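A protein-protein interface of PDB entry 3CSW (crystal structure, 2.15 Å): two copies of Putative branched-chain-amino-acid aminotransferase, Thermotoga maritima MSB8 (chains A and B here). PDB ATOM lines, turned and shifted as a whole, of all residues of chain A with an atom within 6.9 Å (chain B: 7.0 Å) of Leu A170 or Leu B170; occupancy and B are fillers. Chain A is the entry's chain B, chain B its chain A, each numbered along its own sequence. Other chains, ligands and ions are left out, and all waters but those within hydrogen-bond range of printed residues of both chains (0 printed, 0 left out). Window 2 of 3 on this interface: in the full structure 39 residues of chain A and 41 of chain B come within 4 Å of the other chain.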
ATOM      1  N   ARG A 133      -7.392 -23.604  -8.718  1.00  0.00           N
ATOM      2  CA  ARG A 133      -7.491 -22.185  -8.385  1.00  0.00           C
ATOM      3  C   ARG A 133      -8.454 -21.475  -9.343  1.00  0.00           C
ATOM      4  O   ARG A 133      -8.477 -21.728 -10.541  1.00  0.00           O
ATOM      5  CB  ARG A 133      -6.119 -21.502  -8.403  1.00  0.00           C
ATOM      6  CG  ARG A 133      -5.095 -22.045  -7.390  1.00  0.00           C
ATOM      7  CD  ARG A 133      -5.601 -22.068  -5.949  1.00  0.00           C
ATOM      8  NE  ARG A 133      -4.564 -22.619  -5.104  1.00  0.00           N
ATOM      9  CZ  ARG A 133      -3.567 -21.925  -4.553  1.00  0.00           C
ATOM     10  NH1 ARG A 133      -3.466 -20.616  -4.687  1.00  0.00           N
ATOM     11  NH2 ARG A 133      -2.630 -22.563  -3.879  1.00  0.00           N
ATOM     12  N   ARG A 134      -9.219 -20.556  -8.785  1.00  0.00           N
ATOM     13  CA  ARG A 134     -10.149 -19.713  -9.518  1.00  0.00           C
ATOM     14  C   ARG A 134      -9.372 -18.949 -10.590  1.00  0.00           C
ATOM     15  O   ARG A 134      -8.302 -18.372 -10.303  1.00  0.00           O
ATOM     16  CB  ARG A 134     -10.863 -18.787  -8.511  1.00  0.00           C
ATOM     17  CG  ARG A 134     -12.080 -17.986  -9.001  1.00  0.00           C
ATOM     18  CD  ARG A 134     -11.721 -16.638  -9.635  1.00  0.00           C
ATOM     19  NE  ARG A 134     -11.239 -15.675  -8.661  1.00  0.00           N
ATOM     20  CZ  ARG A 134     -10.344 -14.706  -8.887  1.00  0.00           C
ATOM     21  NH1 ARG A 134      -9.764 -14.518 -10.060  1.00  0.00           N
ATOM     22  NH2 ARG A 134      -9.992 -13.921  -7.890  1.00  0.00           N
ATOM     23  N   ILE A 135      -9.912 -18.981 -11.818  1.00  0.00           N
ATOM     24  CA  ILE A 135      -9.258 -18.425 -13.011  1.00  0.00           C
ATOM     25  C   ILE A 135      -8.987 -16.955 -12.757  1.00  0.00           C
ATOM     26  O   ILE A 135      -9.865 -16.227 -12.313  1.00  0.00           O
ATOM     27  CB  ILE A 135     -10.142 -18.636 -14.304  1.00  0.00           C
ATOM     28  CG1 ILE A 135     -10.223 -20.121 -14.671  1.00  0.00           C
ATOM     29  CG2 ILE A 135      -9.663 -17.833 -15.475  1.00  0.00           C
ATOM     30  CD1 ILE A 135     -11.387 -20.442 -15.596  1.00  0.00           C
ATOM     31  N   PRO A 136      -7.765 -16.497 -13.045  1.00  0.00           N
ATOM     32  CA  PRO A 136      -7.508 -15.085 -12.812  1.00  0.00           C
ATOM     33  C   PRO A 136      -8.334 -14.148 -13.717  1.00  0.00           C
ATOM     34  O   PRO A 136      -8.705 -14.520 -14.836  1.00  0.00           O
ATOM     35  CB  PRO A 136      -6.033 -14.939 -13.162  1.00  0.00           C
ATOM     36  CG  PRO A 136      -5.745 -16.053 -14.112  1.00  0.00           C
ATOM     37  CD  PRO A 136      -6.598 -17.185 -13.625  1.00  0.00           C
ATOM     38  N   ASP A 137      -8.536 -12.927 -13.218  1.00  0.00           N
ATOM     39  CA  ASP A 137      -9.283 -11.861 -13.854  1.00  0.00           C
ATOM     40  C   ASP A 137      -8.687 -11.470 -15.209  1.00  0.00           C
ATOM     41  O   ASP A 137      -9.399 -11.059 -16.109  1.00  0.00           O
ATOM     42  CB  ASP A 137      -9.297 -10.648 -12.896  1.00  0.00           C
ATOM     43  CG  ASP A 137     -10.122  -9.482 -13.433  1.00  0.00           C
ATOM     44  OD1 ASP A 137     -11.359  -9.641 -13.618  1.00  0.00           O
ATOM     45  OD2 ASP A 137      -9.528  -8.403 -13.689  1.00  0.00           O
ATOM     46  N   LEU A 138      -7.384 -11.611 -15.361  1.00  0.00           N
ATOM     47  CA  LEU A 138      -6.723 -11.348 -16.639  1.00  0.00           C
ATOM     48  C   LEU A 138      -7.095 -12.379 -17.728  1.00  0.00           C
ATOM     49  O   LEU A 138      -6.889 -12.122 -18.907  1.00  0.00           O
ATOM     50  CB  LEU A 138      -5.202 -11.197 -16.449  1.00  0.00           C
ATOM     51  CG  LEU A 138      -4.648  -9.864 -15.879  1.00  0.00           C
ATOM     52  CD1 LEU A 138      -3.139  -9.909 -15.487  1.00  0.00           C
ATOM     53  CD2 LEU A 138      -4.841  -8.721 -16.875  1.00  0.00           C
ATOM     54  N   SER A 139      -7.729 -13.493 -17.334  1.00  0.00           N
ATOM     55  CA  SER A 139      -8.096 -14.575 -18.255  1.00  0.00           C
ATOM     56  C   SER A 139      -9.606 -14.692 -18.480  1.00  0.00           C
ATOM     57  O   SER A 139     -10.034 -15.027 -19.573  1.00  0.00           O
ATOM     58  CB  SER A 139      -7.597 -15.937 -17.727  1.00  0.00           C
ATOM     59  OG  SER A 139      -6.210 -16.032 -17.678  1.00  0.00           O
ATOM     60  N   LEU A 168      -9.909 -21.561  -4.051  1.00  0.00           N
ATOM     61  CA  LEU A 168      -9.123 -20.421  -3.676  1.00  0.00           C
ATOM     62  C   LEU A 168      -8.699 -19.680  -4.949  1.00  0.00           C
ATOM     63  O   LEU A 168      -8.654 -20.249  -6.034  1.00  0.00           O
ATOM     64  CB  LEU A 168      -7.844 -20.889  -2.927  1.00  0.00           C
ATOM     65  CG  LEU A 168      -8.010 -21.875  -1.778  1.00  0.00           C
ATOM     66  CD1 LEU A 168      -6.656 -22.187  -1.181  1.00  0.00           C
ATOM     67  CD2 LEU A 168      -9.017 -21.333  -0.724  1.00  0.00           C
ATOM     68  N   GLY A 169      -8.311 -18.427  -4.792  1.00  0.00           N
ATOM     69  CA  GLY A 169      -7.725 -17.679  -5.870  1.00  0.00           C
ATOM     70  C   GLY A 169      -6.230 -17.955  -5.900  1.00  0.00           C
ATOM     71  O   GLY A 169      -5.662 -18.584  -5.022  1.00  0.00           O
ATOM     72  N   LEU A 170      -5.591 -17.482  -6.932  1.00  0.00           N
ATOM     73  CA  LEU A 170      -4.169 -17.696  -7.110  1.00  0.00           C
ATOM     74  C   LEU A 170      -3.330 -17.331  -5.907  1.00  0.00           C
ATOM     75  O   LEU A 170      -2.275 -17.918  -5.707  1.00  0.00           O
ATOM     76  CB  LEU A 170      -3.677 -16.979  -8.363  1.00  0.00           C
ATOM     77  CG  LEU A 170      -4.130 -17.606  -9.697  1.00  0.00           C
ATOM     78  CD1 LEU A 170      -3.692 -16.696 -10.853  1.00  0.00           C
ATOM     79  CD2 LEU A 170      -3.596 -19.048  -9.887  1.00  0.00           C
ATOM     80  N   ASN A 171      -3.771 -16.360  -5.114  1.00  0.00           N
ATOM     81  CA  ASN A 171      -3.010 -15.932  -3.946  1.00  0.00           C
ATOM     82  C   ASN A 171      -3.337 -16.649  -2.643  1.00  0.00           C
ATOM     83  O   ASN A 171      -2.696 -16.369  -1.654  1.00  0.00           O
ATOM     84  CB  ASN A 171      -3.130 -14.419  -3.716  1.00  0.00           C
ATOM     85  CG  ASN A 171      -2.558 -13.625  -4.833  1.00  0.00           C
ATOM     86  OD1 ASN A 171      -3.289 -12.919  -5.487  1.00  0.00           O
ATOM     87  ND2 ASN A 171      -1.241 -13.741  -5.076  1.00  0.00           N
ATOM     88  N   GLY A 172      -4.287 -17.579  -2.647  1.00  0.00           N
ATOM     89  CA  GLY A 172      -4.669 -18.297  -1.423  1.00  0.00           C
ATOM     90  C   GLY A 172      -5.866 -17.711  -0.688  1.00  0.00           C
ATOM     91  O   GLY A 172      -6.234 -18.186   0.393  1.00  0.00           O
ATOM     92  N   GLN A 173      -6.475 -16.666  -1.240  1.00  0.00           N
ATOM     93  CA  GLN A 173      -7.704 -16.141  -0.653  1.00  0.00           C
ATOM     94  C   GLN A 173      -8.850 -17.092  -0.984  1.00  0.00           C
ATOM     95  O   GLN A 173      -8.828 -17.734  -2.033  1.00  0.00           O
ATOM     96  CB  GLN A 173      -7.985 -14.711  -1.140  1.00  0.00           C
ATOM     97  CG  GLN A 173      -8.587 -14.567  -2.541  1.00  0.00           C
ATOM     98  CD  GLN A 173      -7.581 -14.649  -3.654  1.00  0.00           C
ATOM     99  OE1 GLN A 173      -6.478 -15.203  -3.504  1.00  0.00           O
ATOM    100  NE2 GLN A 173      -7.960 -14.097  -4.806  1.00  0.00           N
ATOM    101  N   CYS A 175     -12.428 -17.885  -2.348  1.00  0.00           N
ATOM    102  CA  CYS A 175     -13.397 -17.324  -3.298  1.00  0.00           C
ATOM    103  C   CYS A 175     -14.770 -17.959  -3.132  1.00  0.00           C
ATOM    104  O   CYS A 175     -15.724 -17.301  -2.721  1.00  0.00           O
ATOM    105  CB  CYS A 175     -12.889 -17.501  -4.745  1.00  0.00           C
ATOM    106  SG  CYS A 175     -11.390 -16.589  -5.041  1.00  0.00           S
ATOM    107  N   ARG B 133      -5.479 -13.275 -21.283  1.00  0.00           N
ATOM    108  CA  ARG B 133      -4.276 -14.010 -20.926  1.00  0.00           C
ATOM    109  C   ARG B 133      -4.599 -15.484 -20.834  1.00  0.00           C
ATOM    110  O   ARG B 133      -5.683 -15.865 -20.428  1.00  0.00           O
ATOM    111  CB  ARG B 133      -3.654 -13.544 -19.610  1.00  0.00           C
ATOM    112  CG  ARG B 133      -3.207 -12.109 -19.561  1.00  0.00           C
ATOM    113  CD  ARG B 133      -2.108 -11.828 -20.561  1.00  0.00           C
ATOM    114  NE  ARG B 133      -1.761 -10.411 -20.507  1.00  0.00           N
ATOM    115  CZ  ARG B 133      -0.753  -9.869 -19.827  1.00  0.00           C
ATOM    116  NH1 ARG B 133       0.114 -10.605 -19.124  1.00  0.00           N
ATOM    117  NH2 ARG B 133      -0.607  -8.544 -19.848  1.00  0.00           N
ATOM    118  N   ARG B 134      -3.641 -16.307 -21.236  1.00  0.00           N
ATOM    119  CA  ARG B 134      -3.756 -17.762 -21.152  1.00  0.00           C
ATOM    120  C   ARG B 134      -3.933 -18.189 -19.691  1.00  0.00           C
ATOM    121  O   ARG B 134      -3.236 -17.685 -18.816  1.00  0.00           O
ATOM    122  CB  ARG B 134      -2.508 -18.399 -21.745  1.00  0.00           C
ATOM    123  CG  ARG B 134      -2.604 -19.889 -22.035  1.00  0.00           C
ATOM    124  CD  ARG B 134      -3.362 -20.106 -23.323  1.00  0.00           C
ATOM    125  NE  ARG B 134      -3.139 -21.429 -23.886  1.00  0.00           N
ATOM    126  CZ  ARG B 134      -4.015 -22.430 -23.924  1.00  0.00           C
ATOM    127  NH1 ARG B 134      -5.225 -22.328 -23.411  1.00  0.00           N
ATOM    128  NH2 ARG B 134      -3.667 -23.570 -24.507  1.00  0.00           N
ATOM    129  N   ILE B 135      -4.869 -19.120 -19.438  1.00  0.00           N
ATOM    130  CA  ILE B 135      -5.153 -19.576 -18.077  1.00  0.00           C
ATOM    131  C   ILE B 135      -3.923 -20.323 -17.576  1.00  0.00           C
ATOM    132  O   ILE B 135      -3.374 -21.174 -18.310  1.00  0.00           O
ATOM    133  CB  ILE B 135      -6.406 -20.517 -17.985  1.00  0.00           C
ATOM    134  CG1 ILE B 135      -7.678 -19.786 -18.423  1.00  0.00           C
ATOM    135  CG2 ILE B 135      -6.537 -21.086 -16.553  1.00  0.00           C
ATOM    136  CD1 ILE B 135      -8.951 -20.715 -18.523  1.00  0.00           C
ATOM    137  N   PRO B 136      -3.472 -20.002 -16.348  1.00  0.00           N
ATOM    138  CA  PRO B 136      -2.263 -20.644 -15.833  1.00  0.00           C
ATOM    139  C   PRO B 136      -2.551 -22.061 -15.341  1.00  0.00           C
ATOM    140  O   PRO B 136      -3.695 -22.384 -15.037  1.00  0.00           O
ATOM    141  CB  PRO B 136      -1.843 -19.716 -14.675  1.00  0.00           C
ATOM    142  CG  PRO B 136      -3.117 -19.175 -14.160  1.00  0.00           C
ATOM    143  CD  PRO B 136      -4.013 -19.023 -15.387  1.00  0.00           C
ATOM    144  N   ASP B 137      -1.500 -22.868 -15.255  1.00  0.00           N
ATOM    145  CA  ASP B 137      -1.568 -24.259 -14.811  1.00  0.00           C
ATOM    146  C   ASP B 137      -2.268 -24.483 -13.459  1.00  0.00           C
ATOM    147  O   ASP B 137      -2.953 -25.483 -13.288  1.00  0.00           O
ATOM    148  CB  ASP B 137      -0.133 -24.874 -14.785  1.00  0.00           C
ATOM    149  CG  ASP B 137      -0.149 -26.406 -14.731  1.00  0.00           C
ATOM    150  OD1 ASP B 137      -0.801 -27.054 -15.591  1.00  0.00           O
ATOM    151  OD2 ASP B 137       0.496 -26.973 -13.817  1.00  0.00           O
ATOM    152  N   LEU B 138      -2.113 -23.580 -12.497  1.00  0.00           N
ATOM    153  CA  LEU B 138      -2.808 -23.721 -11.193  1.00  0.00           C
ATOM    154  C   LEU B 138      -4.338 -23.672 -11.287  1.00  0.00           C
ATOM    155  O   LEU B 138      -5.029 -24.134 -10.382  1.00  0.00           O
ATOM    156  CB  LEU B 138      -2.333 -22.677 -10.181  1.00  0.00           C
ATOM    157  CG  LEU B 138      -1.016 -22.934  -9.446  1.00  0.00           C
ATOM    158  CD1 LEU B 138      -0.600 -21.663  -8.697  1.00  0.00           C
ATOM    159  CD2 LEU B 138      -1.090 -24.135  -8.510  1.00  0.00           C
ATOM    160  N   SER B 139      -4.850 -23.133 -12.387  1.00  0.00           N
ATOM    161  CA  SER B 139      -6.297 -23.037 -12.643  1.00  0.00           C
ATOM    162  C   SER B 139      -6.844 -24.083 -13.628  1.00  0.00           C
ATOM    163  O   SER B 139      -8.005 -24.495 -13.535  1.00  0.00           O
ATOM    164  CB  SER B 139      -6.609 -21.639 -13.193  1.00  0.00           C
ATOM    165  OG  SER B 139      -6.399 -20.638 -12.223  1.00  0.00           O
ATOM    166  N   LEU B 168      -0.864 -13.971 -24.420  1.00  0.00           N
ATOM    167  CA  LEU B 168       0.278 -13.935 -23.550  1.00  0.00           C
ATOM    168  C   LEU B 168      -0.123 -14.631 -22.258  1.00  0.00           C
ATOM    169  O   LEU B 168      -1.312 -14.696 -21.917  1.00  0.00           O
ATOM    170  CB  LEU B 168       0.684 -12.490 -23.220  1.00  0.00           C
ATOM    171  CG  LEU B 168       0.837 -11.510 -24.386  1.00  0.00           C
ATOM    172  CD1 LEU B 168       1.283 -10.177 -23.872  1.00  0.00           C
ATOM    173  CD2 LEU B 168       1.761 -12.060 -25.432  1.00  0.00           C
ATOM    174  N   GLY B 169       0.865 -15.146 -21.546  1.00  0.00           N
ATOM    175  CA  GLY B 169       0.631 -15.714 -20.226  1.00  0.00           C
ATOM    176  C   GLY B 169       0.563 -14.600 -19.214  1.00  0.00           C
ATOM    177  O   GLY B 169       0.800 -13.439 -19.553  1.00  0.00           O
ATOM    178  N   LEU B 170       0.296 -14.940 -17.955  1.00  0.00           N
ATOM    179  CA  LEU B 170       0.118 -13.924 -16.928  1.00  0.00           C
ATOM    180  C   LEU B 170       1.313 -13.015 -16.751  1.00  0.00           C
ATOM    181  O   LEU B 170       1.137 -11.917 -16.287  1.00  0.00           O
ATOM    182  CB  LEU B 170      -0.215 -14.527 -15.559  1.00  0.00           C
ATOM    183  CG  LEU B 170      -1.604 -15.111 -15.295  1.00  0.00           C
ATOM    184  CD1 LEU B 170      -1.698 -15.489 -13.791  1.00  0.00           C
ATOM    185  CD2 LEU B 170      -2.726 -14.158 -15.743  1.00  0.00           C
ATOM    186  N   ASN B 171       2.528 -13.482 -17.049  1.00  0.00           N
ATOM    187  CA  ASN B 171       3.709 -12.638 -16.892  1.00  0.00           C
ATOM    188  C   ASN B 171       4.145 -11.918 -18.177  1.00  0.00           C
ATOM    189  O   ASN B 171       5.214 -11.316 -18.211  1.00  0.00           O
ATOM    190  CB  ASN B 171       4.907 -13.459 -16.392  1.00  0.00           C
ATOM    191  CG  ASN B 171       4.683 -14.078 -15.018  1.00  0.00           C
ATOM    192  OD1 ASN B 171       4.671 -15.287 -14.895  1.00  0.00           O
ATOM    193  ND2 ASN B 171       4.534 -13.247 -13.990  1.00  0.00           N
ATOM    194  N   GLY B 172       3.352 -11.966 -19.240  1.00  0.00           N
ATOM    195  CA  GLY B 172       3.763 -11.308 -20.469  1.00  0.00           C
ATOM    196  C   GLY B 172       4.627 -12.142 -21.403  1.00  0.00           C
ATOM    197  O   GLY B 172       5.110 -11.627 -22.411  1.00  0.00           O
ATOM    198  N   GLN B 173       4.820 -13.422 -21.074  1.00  0.00           N
ATOM    199  CA  GLN B 173       5.459 -14.362 -21.988  1.00  0.00           C
ATOM    200  C   GLN B 173       4.491 -14.664 -23.117  1.00  0.00           C
ATOM    201  O   GLN B 173       3.290 -14.676 -22.915  1.00  0.00           O
ATOM    202  CB  GLN B 173       5.907 -15.664 -21.282  1.00  0.00           C
ATOM    203  CG  GLN B 173       4.825 -16.704 -20.927  1.00  0.00           C
ATOM    204  CD  GLN B 173       4.101 -16.441 -19.607  1.00  0.00           C
ATOM    205  OE1 GLN B 173       4.023 -15.313 -19.137  1.00  0.00           O
ATOM    206  NE2 GLN B 173       3.557 -17.493 -19.023  1.00  0.00           N
ATOM    207  N   CYS B 175       2.514 -17.065 -25.269  1.00  0.00           N
ATOM    208  CA  CYS B 175       2.035 -18.447 -25.203  1.00  0.00           C
ATOM    209  C   CYS B 175       1.767 -18.923 -26.618  1.00  0.00           C
ATOM    210  O   CYS B 175       2.574 -19.658 -27.206  1.00  0.00           O
ATOM    211  CB  CYS B 175       0.804 -18.577 -24.281  1.00  0.00           C
ATOM    212  SG  CYS B 175       1.281 -18.461 -22.530  1.00  0.00           S
ATOM    213  N   SER B 197       6.032 -22.719 -20.908  1.00  0.00           N
ATOM    214  CA  SER B 197       5.469 -21.383 -20.954  1.00  0.00           C
ATOM    215  C   SER B 197       3.969 -21.451 -20.674  1.00  0.00           C
ATOM    216  O   SER B 197       3.369 -20.473 -20.233  1.00  0.00           O
ATOM    217  CB  SER B 197       5.705 -20.744 -22.316  1.00  0.00           C
ATOM    218  OG  SER B 197       7.080 -20.555 -22.572  1.00  0.00           O
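Ile A135 touches Ile B135. OG of Ser B139 touches CA of Ile A135, 3.7 Å away. Pro B136 touches Pro A136. Ser B139 touches Pro A136 (OG to CD, 3.7 Å). Leu B170 touches Pro A136. CB of Leu A138 touches CD2 of Leu B170, at 3.9 Å. Ser A139 touches Arg B134 (OG to O, 3.6 Å). Ser A139 touches Ile B135. Leu B138 touches Leu A170 (CB to CD2, 3.9 Å). Leu A170 touches Leu B170.
Of the 14 printed residues of chain A, 7 touch a printed residue of chain B. Hydrophobic or aromatic side chains of chain B that line the printed part of chain A: Ile B135, Pro B136, Leu B138 and Leu B170. Among the printed residues, no Asp or Glu carboxylate lies within 4 Å of a Lys or Arg side-chain nitrogen of the other chain.
O of Leu B168 is in hydrogen-bond range of N of Arg B134. The guanidinium group of Arg B133 is in hydrogen-bond range of the backbone carbonyl oxygen of Gly B169 (2.9 Å). The guanidinium group (NH1) of Arg A133 is in hydrogen-bond range of the backbone carbonyl oxygen (O) of Leu A170 (3.1 Å). O of Leu A168 sits at hydrogen-bond distance from N of Arg A134, 2.8 Å away. The guanidinium group (NE) of Arg A134 lies within hydrogen-bond range of the side-chain sulfur (SG) of Cys A175. NH1 of Arg A133 lies within hydrogen-bond range of O of Gly A169, 3.0 Å away.
Arg A133 touches Ser B139, and with the chains exchanged Ser A139 touches Arg B133. Arg A134 touches Ser B139, and with the chains exchanged Ser A139 touches Arg B134. Pro A136 touches Ser B139, but with the chains exchanged Ser A139 does not touch Pro B136 (4.4 Å). Leu B170 touches its own counterpart, Leu A170. Of the 16 pairs that touch across the chains among the printed residues, 13 have their exchanged pair printed and touching as well.
The side-chain hydroxyl (OG) of Ser B139 lies within hydrogen-bond range of the backbone carbonyl oxygen (O) of Arg A133 (2.9 Å). The backbone carbonyl oxygen (O) of Arg B133 lies within hydrogen-bond range of the side-chain hydroxyl (OG) of Ser A139 (2.8 Å). The backbone carbonyl oxygen (O) of Leu A138 is in hydrogen-bond range of the backbone NH (N) of Arg B133 (3.0 Å). The backbone carbonyl oxygen (O) of Leu B138 is in hydrogen-bond range of the backbone NH (N) of Arg A133, 2.9 Å away.
Printed residues of chain B within 4 Å of Leu A138: Arg B133 (3.0 Å) and Leu B170 (3.9 Å). Leu A168 touches none of the printed residues of chain B. Of the printed residues of chain B, Leu A170 touches Leu B138 (3.9 Å), Ser B139 (3.98 Å) and Leu B170 (3.8 Å). Of the printed residues of chain A, Leu B138 touches Arg A133 (2.9 Å) and Leu A170 (3.9 Å). Of chain A, only Pro A136 (3.9 Å), Leu A138 (3.9 Å) and Leu A170 (3.8 Å) come within 4 Å of Leu B170. Gln B173 touches none of the printed residues of chain A. The nearest printed residue of chain B that does not touch Leu A170 is Pro B136 (4.2 Å). The nearest residue of chain A that does not touch Leu B170 is Ser A139 (4.4 Å). The nearest printed residue of chain B that does not touch Arg A133 is Ile B135 (6.3 Å).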
